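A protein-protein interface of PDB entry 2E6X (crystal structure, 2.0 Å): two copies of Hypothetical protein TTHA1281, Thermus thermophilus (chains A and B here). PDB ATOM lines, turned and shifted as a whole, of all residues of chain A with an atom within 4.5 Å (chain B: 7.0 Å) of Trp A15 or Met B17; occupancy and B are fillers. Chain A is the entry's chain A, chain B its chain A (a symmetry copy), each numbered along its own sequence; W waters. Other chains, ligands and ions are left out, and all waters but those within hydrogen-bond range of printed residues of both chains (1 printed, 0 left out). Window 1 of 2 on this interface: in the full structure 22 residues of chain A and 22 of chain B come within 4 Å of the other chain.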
ATOM      1  N   GLU A   2      -7.449 -16.049 -20.384  1.00  0.00           N
ATOM      2  CA  GLU A   2      -8.188 -17.087 -19.653  1.00  0.00           C
ATOM      3  C   GLU A   2      -7.361 -18.254 -19.114  1.00  0.00           C
ATOM      4  O   GLU A   2      -7.544 -18.649 -17.979  1.00  0.00           O
ATOM      5  CB  GLU A   2      -9.305 -17.652 -20.538  1.00  0.00           C
ATOM      6  CG  GLU A   2     -10.226 -18.635 -19.813  1.00  0.00           C
ATOM      7  CD  GLU A   2     -11.082 -17.974 -18.762  1.00  0.00           C
ATOM      8  OE1 GLU A   2     -11.733 -18.712 -17.969  1.00  0.00           O
ATOM      9  OE2 GLU A   2     -11.109 -16.710 -18.731  1.00  0.00           O
ATOM     10  N   LEU A  13      -8.329 -26.835 -18.208  1.00  0.00           N
ATOM     11  CA  LEU A  13      -9.414 -27.299 -19.075  1.00  0.00           C
ATOM     12  C   LEU A  13      -8.855 -28.294 -20.088  1.00  0.00           C
ATOM     13  O   LEU A  13      -7.735 -28.129 -20.573  1.00  0.00           O
ATOM     14  CB  LEU A  13     -10.018 -26.107 -19.827  1.00  0.00           C
ATOM     15  CG  LEU A  13     -10.601 -24.978 -18.983  1.00  0.00           C
ATOM     16  CD1 LEU A  13     -11.131 -23.925 -19.915  1.00  0.00           C
ATOM     17  CD2 LEU A  13     -11.722 -25.499 -18.096  1.00  0.00           C
ATOM     18  N   VAL A  14      -9.629 -29.326 -20.399  1.00  0.00           N
ATOM     19  CA  VAL A  14      -9.201 -30.326 -21.367  1.00  0.00           C
ATOM     20  C   VAL A  14      -9.952 -30.033 -22.646  1.00  0.00           C
ATOM     21  O   VAL A  14     -11.153 -29.756 -22.615  1.00  0.00           O
ATOM     22  CB  VAL A  14      -9.553 -31.749 -20.921  1.00  0.00           C
ATOM     23  CG1 VAL A  14      -8.872 -32.781 -21.844  1.00  0.00           C
ATOM     24  CG2 VAL A  14      -9.139 -31.945 -19.468  1.00  0.00           C
ATOM     25  N   TRP A  15      -9.229 -30.069 -23.757  1.00  0.00           N
ATOM     26  CA  TRP A  15      -9.799 -29.820 -25.070  1.00  0.00           C
ATOM     27  C   TRP A  15      -9.567 -30.989 -26.011  1.00  0.00           C
ATOM     28  O   TRP A  15      -8.456 -31.534 -26.064  1.00  0.00           O
ATOM     29  CB  TRP A  15      -9.163 -28.593 -25.718  1.00  0.00           C
ATOM     30  CG  TRP A  15      -9.460 -27.325 -25.032  1.00  0.00           C
ATOM     31  CD1 TRP A  15      -8.763 -26.764 -23.993  1.00  0.00           C
ATOM     32  CD2 TRP A  15     -10.571 -26.464 -25.284  1.00  0.00           C
ATOM     33  NE1 TRP A  15      -9.381 -25.605 -23.584  1.00  0.00           N
ATOM     34  CE2 TRP A  15     -10.493 -25.400 -24.358  1.00  0.00           C
ATOM     35  CE3 TRP A  15     -11.632 -26.490 -26.198  1.00  0.00           C
ATOM     36  CZ2 TRP A  15     -11.433 -24.369 -24.325  1.00  0.00           C
ATOM     37  CZ3 TRP A  15     -12.572 -25.456 -26.160  1.00  0.00           C
ATOM     38  CH2 TRP A  15     -12.463 -24.413 -25.228  1.00  0.00           C
ATOM     39  N   ARG A  16     -10.617 -31.375 -26.751  1.00  0.00           N
ATOM     40  CA  ARG A  16     -10.534 -32.442 -27.746  1.00  0.00           C
ATOM     41  C   ARG A  16     -11.402 -32.002 -28.911  1.00  0.00           C
ATOM     42  O   ARG A  16     -12.436 -31.349 -28.719  1.00  0.00           O
ATOM     43  CB  ARG A  16     -11.072 -33.777 -27.211  1.00  0.00           C
ATOM     44  CG  ARG A  16     -10.261 -34.410 -26.042  1.00  0.00           C
ATOM     45  CD  ARG A  16      -8.881 -34.900 -26.472  1.00  0.00           C
ATOM     46  NE  ARG A  16      -8.222 -35.611 -25.369  1.00  0.00           N
ATOM     47  CZ  ARG A  16      -7.459 -35.034 -24.443  1.00  0.00           C
ATOM     48  NH1 ARG A  16      -7.232 -33.725 -24.488  1.00  0.00           N
ATOM     49  NH2 ARG A  16      -6.954 -35.771 -23.450  1.00  0.00           N
ATOM     50  N   VAL A  28     -16.158 -29.697 -30.797  1.00  0.00           N
ATOM     51  CA  VAL A  28     -15.145 -29.319 -29.822  1.00  0.00           C
ATOM     52  C   VAL A  28     -15.676 -29.746 -28.468  1.00  0.00           C
ATOM     53  O   VAL A  28     -16.829 -29.404 -28.082  1.00  0.00           O
ATOM     54  CB  VAL A  28     -14.882 -27.823 -29.858  1.00  0.00           C
ATOM     55  CG1 VAL A  28     -14.039 -27.391 -28.643  1.00  0.00           C
ATOM     56  CG2 VAL A  28     -14.148 -27.512 -31.181  1.00  0.00           C
ATOM     57  N   ARG A  29     -14.896 -30.554 -27.765  1.00  0.00           N
ATOM     58  CA  ARG A  29     -15.339 -30.966 -26.439  1.00  0.00           C
ATOM     59  C   ARG A  29     -14.435 -30.302 -25.421  1.00  0.00           C
ATOM     60  O   ARG A  29     -13.210 -30.279 -25.602  1.00  0.00           O
ATOM     61  CB  ARG A  29     -15.294 -32.493 -26.283  1.00  0.00           C
ATOM     62  CG  ARG A  29     -16.254 -33.171 -27.192  1.00  0.00           C
ATOM     63  CD  ARG A  29     -16.080 -34.669 -27.155  1.00  0.00           C
ATOM     64  NE  ARG A  29     -17.157 -35.303 -27.921  1.00  0.00           N
ATOM     65  CZ  ARG A  29     -17.147 -36.571 -28.288  1.00  0.00           C
ATOM     66  NH1 ARG A  29     -16.106 -37.341 -27.950  1.00  0.00           N
ATOM     67  NH2 ARG A  29     -18.154 -37.055 -29.021  1.00  0.00           N
ATOM     68  N   VAL A  30     -15.040 -29.760 -24.367  1.00  0.00           N
ATOM     69  CA  VAL A  30     -14.281 -29.088 -23.312  1.00  0.00           C
ATOM     70  C   VAL A  30     -14.788 -29.418 -21.899  1.00  0.00           C
ATOM     71  O   VAL A  30     -15.995 -29.567 -21.667  1.00  0.00           O
ATOM     72  CB  VAL A  30     -14.305 -27.556 -23.511  1.00  0.00           C
ATOM     73  CG1 VAL A  30     -15.741 -27.009 -23.343  1.00  0.00           C
ATOM     74  CG2 VAL A  30     -13.391 -26.898 -22.498  1.00  0.00           C
ATOM     75  N   MET B   1      -6.290 -39.078 -32.374  1.00  0.00           N
ATOM     76  CA  MET B   1      -6.322 -37.776 -31.655  1.00  0.00           C
ATOM     77  C   MET B   1      -5.819 -36.655 -32.573  1.00  0.00           C
ATOM     78  O   MET B   1      -4.686 -36.702 -33.078  1.00  0.00           O
ATOM     79  CB  MET B   1      -5.451 -37.858 -30.404  1.00  0.00           C
ATOM     80  CG  MET B   1      -5.880 -36.892 -29.319  1.00  0.00           C
ATOM     81  SD  MET B   1      -7.092 -37.727 -28.076  1.00  0.00           S
ATOM     82  CE  MET B   1      -8.676 -37.859 -29.194  1.00  0.00           C
ATOM     83  N   LYS B   3      -4.756 -33.453 -32.123  1.00  0.00           N
ATOM     84  CA  LYS B   3      -3.533 -32.714 -31.773  1.00  0.00           C
ATOM     85  C   LYS B   3      -2.303 -33.499 -32.240  1.00  0.00           C
ATOM     86  O   LYS B   3      -1.357 -32.943 -32.813  1.00  0.00           O
ATOM     87  CB  LYS B   3      -3.499 -32.470 -30.249  1.00  0.00           C
ATOM     88  CG  LYS B   3      -2.357 -31.608 -29.714  1.00  0.00           C
ATOM     89  CD  LYS B   3      -2.591 -31.294 -28.215  1.00  0.00           C
ATOM     90  CE  LYS B   3      -1.426 -30.548 -27.545  1.00  0.00           C
ATOM     91  NZ  LYS B   3      -1.216 -29.174 -28.084  1.00  0.00           N
ATOM     92  N   TRP B  15      -5.287 -21.541 -29.556  1.00  0.00           N
ATOM     93  CA  TRP B  15      -6.608 -21.409 -28.967  1.00  0.00           C
ATOM     94  C   TRP B  15      -6.659 -20.276 -27.957  1.00  0.00           C
ATOM     95  O   TRP B  15      -5.747 -20.138 -27.130  1.00  0.00           O
ATOM     96  CB  TRP B  15      -7.008 -22.683 -28.229  1.00  0.00           C
ATOM     97  CG  TRP B  15      -7.199 -23.852 -29.102  1.00  0.00           C
ATOM     98  CD1 TRP B  15      -6.243 -24.747 -29.508  1.00  0.00           C
ATOM     99  CD2 TRP B  15      -8.415 -24.243 -29.742  1.00  0.00           C
ATOM    100  NE1 TRP B  15      -6.796 -25.669 -30.366  1.00  0.00           N
ATOM    101  CE2 TRP B  15      -8.126 -25.381 -30.527  1.00  0.00           C
ATOM    102  CE3 TRP B  15      -9.722 -23.739 -29.734  1.00  0.00           C
ATOM    103  CZ2 TRP B  15      -9.099 -26.026 -31.293  1.00  0.00           C
ATOM    104  CZ3 TRP B  15     -10.693 -24.388 -30.504  1.00  0.00           C
ATOM    105  CH2 TRP B  15     -10.371 -25.517 -31.271  1.00  0.00           C
ATOM    106  N   ARG B  16      -7.723 -19.463 -28.027  1.00  0.00           N
ATOM    107  CA  ARG B  16      -7.946 -18.367 -27.086  1.00  0.00           C
ATOM    108  C   ARG B  16      -9.441 -18.331 -26.825  1.00  0.00           C
ATOM    109  O   ARG B  16     -10.247 -18.612 -27.723  1.00  0.00           O
ATOM    110  CB  ARG B  16      -7.514 -17.011 -27.662  1.00  0.00           C
ATOM    111  CG  ARG B  16      -5.991 -16.849 -27.936  1.00  0.00           C
ATOM    112  CD  ARG B  16      -5.157 -16.806 -26.658  1.00  0.00           C
ATOM    113  NE  ARG B  16      -3.752 -16.512 -26.971  1.00  0.00           N
ATOM    114  CZ  ARG B  16      -2.830 -17.429 -27.251  1.00  0.00           C
ATOM    115  NH1 ARG B  16      -3.148 -18.720 -27.241  1.00  0.00           N
ATOM    116  NH2 ARG B  16      -1.593 -17.043 -27.576  1.00  0.00           N
ATOM    117  N   MET B  17      -9.832 -17.986 -25.607  1.00  0.00           N
ATOM    118  CA  MET B  17     -11.255 -17.921 -25.310  1.00  0.00           C
ATOM    119  C   MET B  17     -11.547 -16.902 -24.243  1.00  0.00           C
ATOM    120  O   MET B  17     -10.659 -16.495 -23.505  1.00  0.00           O
ATOM    121  CB  MET B  17     -11.736 -19.264 -24.838  1.00  0.00           C
ATOM    122  CG  MET B  17     -10.884 -19.738 -23.714  1.00  0.00           C
ATOM    123  SD  MET B  17     -11.258 -21.528 -23.396  1.00  0.00           S
ATOM    124  CE  MET B  17     -13.205 -21.471 -23.370  1.00  0.00           C
ATOM    125  N   GLY B  18     -12.822 -16.532 -24.155  1.00  0.00           N
ATOM    126  CA  GLY B  18     -13.254 -15.554 -23.182  1.00  0.00           C
ATOM    127  C   GLY B  18     -14.622 -15.039 -23.594  1.00  0.00           C
ATOM    128  O   GLY B  18     -15.159 -15.363 -24.679  1.00  0.00           O
ATOM    129  N   ARG B  19     -15.220 -14.242 -22.728  1.00  0.00           N
ATOM    130  CA  ARG B  19     -16.531 -13.743 -23.054  1.00  0.00           C
ATOM    131  C   ARG B  19     -16.464 -12.520 -23.950  1.00  0.00           C
ATOM    132  O   ARG B  19     -15.542 -11.717 -23.857  1.00  0.00           O
ATOM    133  CB  ARG B  19     -17.326 -13.400 -21.780  1.00  0.00           C
ATOM    134  CG  ARG B  19     -18.850 -13.477 -21.987  1.00  0.00           C
ATOM    135  CD  ARG B  19     -19.612 -12.657 -20.917  1.00  0.00           C
ATOM    136  NE  ARG B  19     -19.600 -11.274 -21.349  1.00  0.00           N
ATOM    137  CZ  ARG B  19     -19.773 -10.213 -20.571  1.00  0.00           C
ATOM    138  NH1 ARG B  19     -19.995 -10.358 -19.254  1.00  0.00           N
ATOM    139  NH2 ARG B  19     -19.681  -8.993 -21.122  1.00  0.00           N
ATOM    140  N   LEU B  26     -19.790 -16.922 -25.072  1.00  0.00           N
ATOM    141  CA  LEU B  26     -18.424 -17.420 -24.927  1.00  0.00           C
ATOM    142  C   LEU B  26     -17.822 -17.463 -26.334  1.00  0.00           C
ATOM    143  O   LEU B  26     -18.404 -18.055 -27.240  1.00  0.00           O
ATOM    144  CB  LEU B  26     -18.378 -18.838 -24.332  1.00  0.00           C
ATOM    145  CG  LEU B  26     -16.939 -19.413 -24.409  1.00  0.00           C
ATOM    146  CD1 LEU B  26     -16.068 -18.724 -23.308  1.00  0.00           C
ATOM    147  CD2 LEU B  26     -16.946 -20.934 -24.211  1.00  0.00           C
ATOM    148  N   VAL B  27     -16.670 -16.820 -26.516  1.00  0.00           N
ATOM    149  CA  VAL B  27     -16.033 -16.832 -27.826  1.00  0.00           C
ATOM    150  C   VAL B  27     -14.788 -17.729 -27.803  1.00  0.00           C
ATOM    151  O   VAL B  27     -13.970 -17.688 -26.869  1.00  0.00           O
ATOM    152  CB  VAL B  27     -15.635 -15.386 -28.275  1.00  0.00           C
ATOM    153  CG1 VAL B  27     -14.862 -15.414 -29.577  1.00  0.00           C
ATOM    154  CG2 VAL B  27     -16.921 -14.492 -28.412  1.00  0.00           C
ATOM    155  N   VAL B  28     -14.696 -18.615 -28.775  1.00  0.00           N
ATOM    156  CA  VAL B  28     -13.501 -19.438 -28.904  1.00  0.00           C
ATOM    157  C   VAL B  28     -12.847 -19.036 -30.211  1.00  0.00           C
ATOM    158  O   VAL B  28     -13.502 -19.013 -31.289  1.00  0.00           O
ATOM    159  CB  VAL B  28     -13.854 -20.916 -28.902  1.00  0.00           C
ATOM    160  CG1 VAL B  28     -12.640 -21.764 -29.329  1.00  0.00           C
ATOM    161  CG2 VAL B  28     -14.311 -21.283 -27.473  1.00  0.00           C
ATOM    162  N   ARG B  29     -11.584 -18.641 -30.131  1.00  0.00           N
ATOM    163  CA  ARG B  29     -10.892 -18.278 -31.362  1.00  0.00           C
ATOM    164  C   ARG B  29      -9.843 -19.337 -31.632  1.00  0.00           C
ATOM    165  O   ARG B  29      -9.128 -19.751 -30.708  1.00  0.00           O
ATOM    166  CB  ARG B  29     -10.241 -16.892 -31.251  1.00  0.00           C
ATOM    167  CG  ARG B  29     -11.254 -15.816 -31.098  1.00  0.00           C
ATOM    168  CD  ARG B  29     -10.602 -14.485 -30.818  1.00  0.00           C
ATOM    169  NE  ARG B  29     -11.617 -13.428 -30.854  1.00  0.00           N
ATOM    170  CZ  ARG B  29     -11.416 -12.203 -30.406  1.00  0.00           C
ATOM    171  NH1 ARG B  29     -10.224 -11.883 -29.889  1.00  0.00           N
ATOM    172  NH2 ARG B  29     -12.414 -11.315 -30.441  1.00  0.00           N
ATOM    173  N   LEU B  45     -11.377 -10.063 -25.560  1.00  0.00           N
ATOM    174  CA  LEU B  45     -12.367 -10.917 -24.872  1.00  0.00           C
ATOM    175  C   LEU B  45     -12.131 -10.822 -23.371  1.00  0.00           C
ATOM    176  O   LEU B  45     -11.017 -10.569 -22.946  1.00  0.00           O
ATOM    177  CB  LEU B  45     -12.198 -12.370 -25.251  1.00  0.00           C
ATOM    178  CG  LEU B  45     -12.402 -12.602 -26.746  1.00  0.00           C
ATOM    179  CD1 LEU B  45     -12.072 -14.038 -27.083  1.00  0.00           C
ATOM    180  CD2 LEU B  45     -13.797 -12.241 -27.135  1.00  0.00           C
ATOM    181  N   LEU B  46     -13.166 -11.088 -22.574  1.00  0.00           N
ATOM    182  CA  LEU B  46     -13.045 -11.017 -21.118  1.00  0.00           C
ATOM    183  C   LEU B  46     -12.867 -12.351 -20.405  1.00  0.00           C
ATOM    184  O   LEU B  46     -13.544 -13.362 -20.742  1.00  0.00           O
ATOM    185  CB  LEU B  46     -14.279 -10.313 -20.540  1.00  0.00           C
ATOM    186  CG  LEU B  46     -14.438  -8.817 -20.869  1.00  0.00           C
ATOM    187  CD1 LEU B  46     -15.785  -8.321 -20.376  1.00  0.00           C
ATOM    188  CD2 LEU B  46     -13.286  -8.016 -20.218  1.00  0.00           C
ATOM    189  N   ASN B  47     -11.975 -12.359 -19.399  1.00  0.00           N
ATOM    190  CA  ASN B  47     -11.781 -13.576 -18.602  1.00  0.00           C
ATOM    191  C   ASN B  47     -13.104 -13.864 -17.914  1.00  0.00           C
ATOM    192  O   ASN B  47     -13.913 -12.953 -17.690  1.00  0.00           O
ATOM    193  CB  ASN B  47     -10.738 -13.388 -17.493  1.00  0.00           C
ATOM    194  CG  ASN B  47      -9.396 -12.950 -18.030  1.00  0.00           C
ATOM    195  OD1 ASN B  47      -8.907 -13.494 -19.023  1.00  0.00           O
ATOM    196  ND2 ASN B  47      -8.795 -11.948 -17.378  1.00  0.00           N
ATOM    197  N   LEU B  48     -13.357 -15.125 -17.604  1.00  0.00           N
ATOM    198  CA  LEU B  48     -14.579 -15.416 -16.869  1.00  0.00           C
ATOM    199  C   LEU B  48     -14.360 -16.708 -16.084  1.00  0.00           C
ATOM    200  O   LEU B  48     -13.496 -17.524 -16.442  1.00  0.00           O
ATOM    201  CB  LEU B  48     -15.802 -15.518 -17.816  1.00  0.00           C
ATOM    202  CG  LEU B  48     -15.834 -16.786 -18.647  1.00  0.00           C
ATOM    203  CD1 LEU B  48     -17.046 -16.758 -19.573  1.00  0.00           C
ATOM    204  CD2 LEU B  48     -14.594 -16.881 -19.458  1.00  0.00           C
ATOM    205  N   MET B  53     -18.176 -20.430 -17.952  1.00  0.00           N
ATOM    206  CA  MET B  53     -17.872 -21.063 -19.234  1.00  0.00           C
ATOM    207  C   MET B  53     -18.705 -22.316 -19.407  1.00  0.00           C
ATOM    208  O   MET B  53     -19.212 -22.566 -20.485  1.00  0.00           O
ATOM    209  CB  MET B  53     -16.391 -21.442 -19.358  1.00  0.00           C
ATOM    210  CG  MET B  53     -15.429 -20.271 -19.463  1.00  0.00           C
ATOM    211  SD  MET B  53     -13.626 -20.916 -19.912  1.00  0.00           S
ATOM    212  CE  MET B  53     -14.152 -22.719 -20.392  1.00  0.00           C
ATOM    213  N   VAL B  57     -21.476 -22.855 -22.481  1.00  0.00           N
ATOM    214  CA  VAL B  57     -21.378 -23.944 -23.445  1.00  0.00           C
ATOM    215  C   VAL B  57     -22.662 -24.749 -23.348  1.00  0.00           C
ATOM    216  O   VAL B  57     -23.295 -25.031 -24.361  1.00  0.00           O
ATOM    217  CB  VAL B  57     -20.157 -24.849 -23.179  1.00  0.00           C
ATOM    218  CG1 VAL B  57     -20.179 -26.071 -24.203  1.00  0.00           C
ATOM    219  CG2 VAL B  57     -18.875 -24.013 -23.381  1.00  0.00           C
HETATM  220  O   HOH W   1      -9.773 -13.860 -21.619  1.00  0.00           O
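Hydrophobic or aromatic side chains of chain B that line the printed part of chain A: Met B1, Met B17, Leu B48 and Met B53. Along chain B the printed residues that touch a printed residue of chain A span positions 1 to 53. Hydrophobic or aromatic side chains of chain A that line the printed part of chain B: Leu A13 and Trp A15. Among the printed residues, 7 pairs touch across the chains. Among the printed residues, no Asp or Glu carboxylate lies within 4 Å of a Lys or Arg side-chain nitrogen of the other chain.
The backbone NH of Arg A29 is in hydrogen-bond range of the backbone carbonyl oxygen of Arg A16 (2.8 Å).
Of chain B, only Met B17 comes within 4 Å of Trp A15. Of chain A, only Glu A2 (3.5 Å) and Trp A15 (3.0 Å) come within 4 Å of Met B17. Printed residues of chain B within 4 Å of Glu A2: Met B17 (3.5 Å), Asn B47 (3.2 Å), Leu B48 (2.6 Å) and Met B53 (3.5 Å). Of the printed residues of chain A, Met B53 touches Glu A2 and Leu A13. Printed residues of chain A within 4 Å of Met B1: Arg A16 (3.6 Å). Printed residues of chain A within 4 Å of Leu B48: Glu A2. Of the printed residues of chain B, Arg A16 touches Met B1 (3.6 Å). Gly B18 touches none of the printed residues of chain A. The nearest residue of chain B that does not touch Trp A15 is Val B28 (4.3 Å). The nearest residue of chain A that does not touch Met B17 is Leu A13 (4.2 Å).
The side-chain sulfur (SD) of Met B53 lies close to the side-chain carboxylate (OE1) of Glu A2 (3.5 Å). The guanidinium group (NE) of Arg A16 is in hydrogen-bond range of the side-chain sulfur (SD) of Met B1 (3.6 Å). The side-chain amide oxygen (OD1) of Asn B47 is in hydrogen-bond range of the backbone NH (N) of Glu A2. N of Leu B48 sits at hydrogen-bond distance from OE2 of Glu A2, 3.0 Å away.
Among the printed residues, merely in contact across the chains: Trp A15 with Met B17, Leu A13 with Met B53 and Glu A2 with Met B17.
Positions printed for both chains: 15, 16, 28 and 29. Of the 7 pairs that touch across the chains among the printed residues, none has its exchanged pair printed and touching as well.
Water W1 lies within hydrogen-bond range of the side-chain amide oxygen (OD1) of Asn B47, the backbone carbonyl oxygen (O) of Met B17 and the backbone NH (N) of Glu A2.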
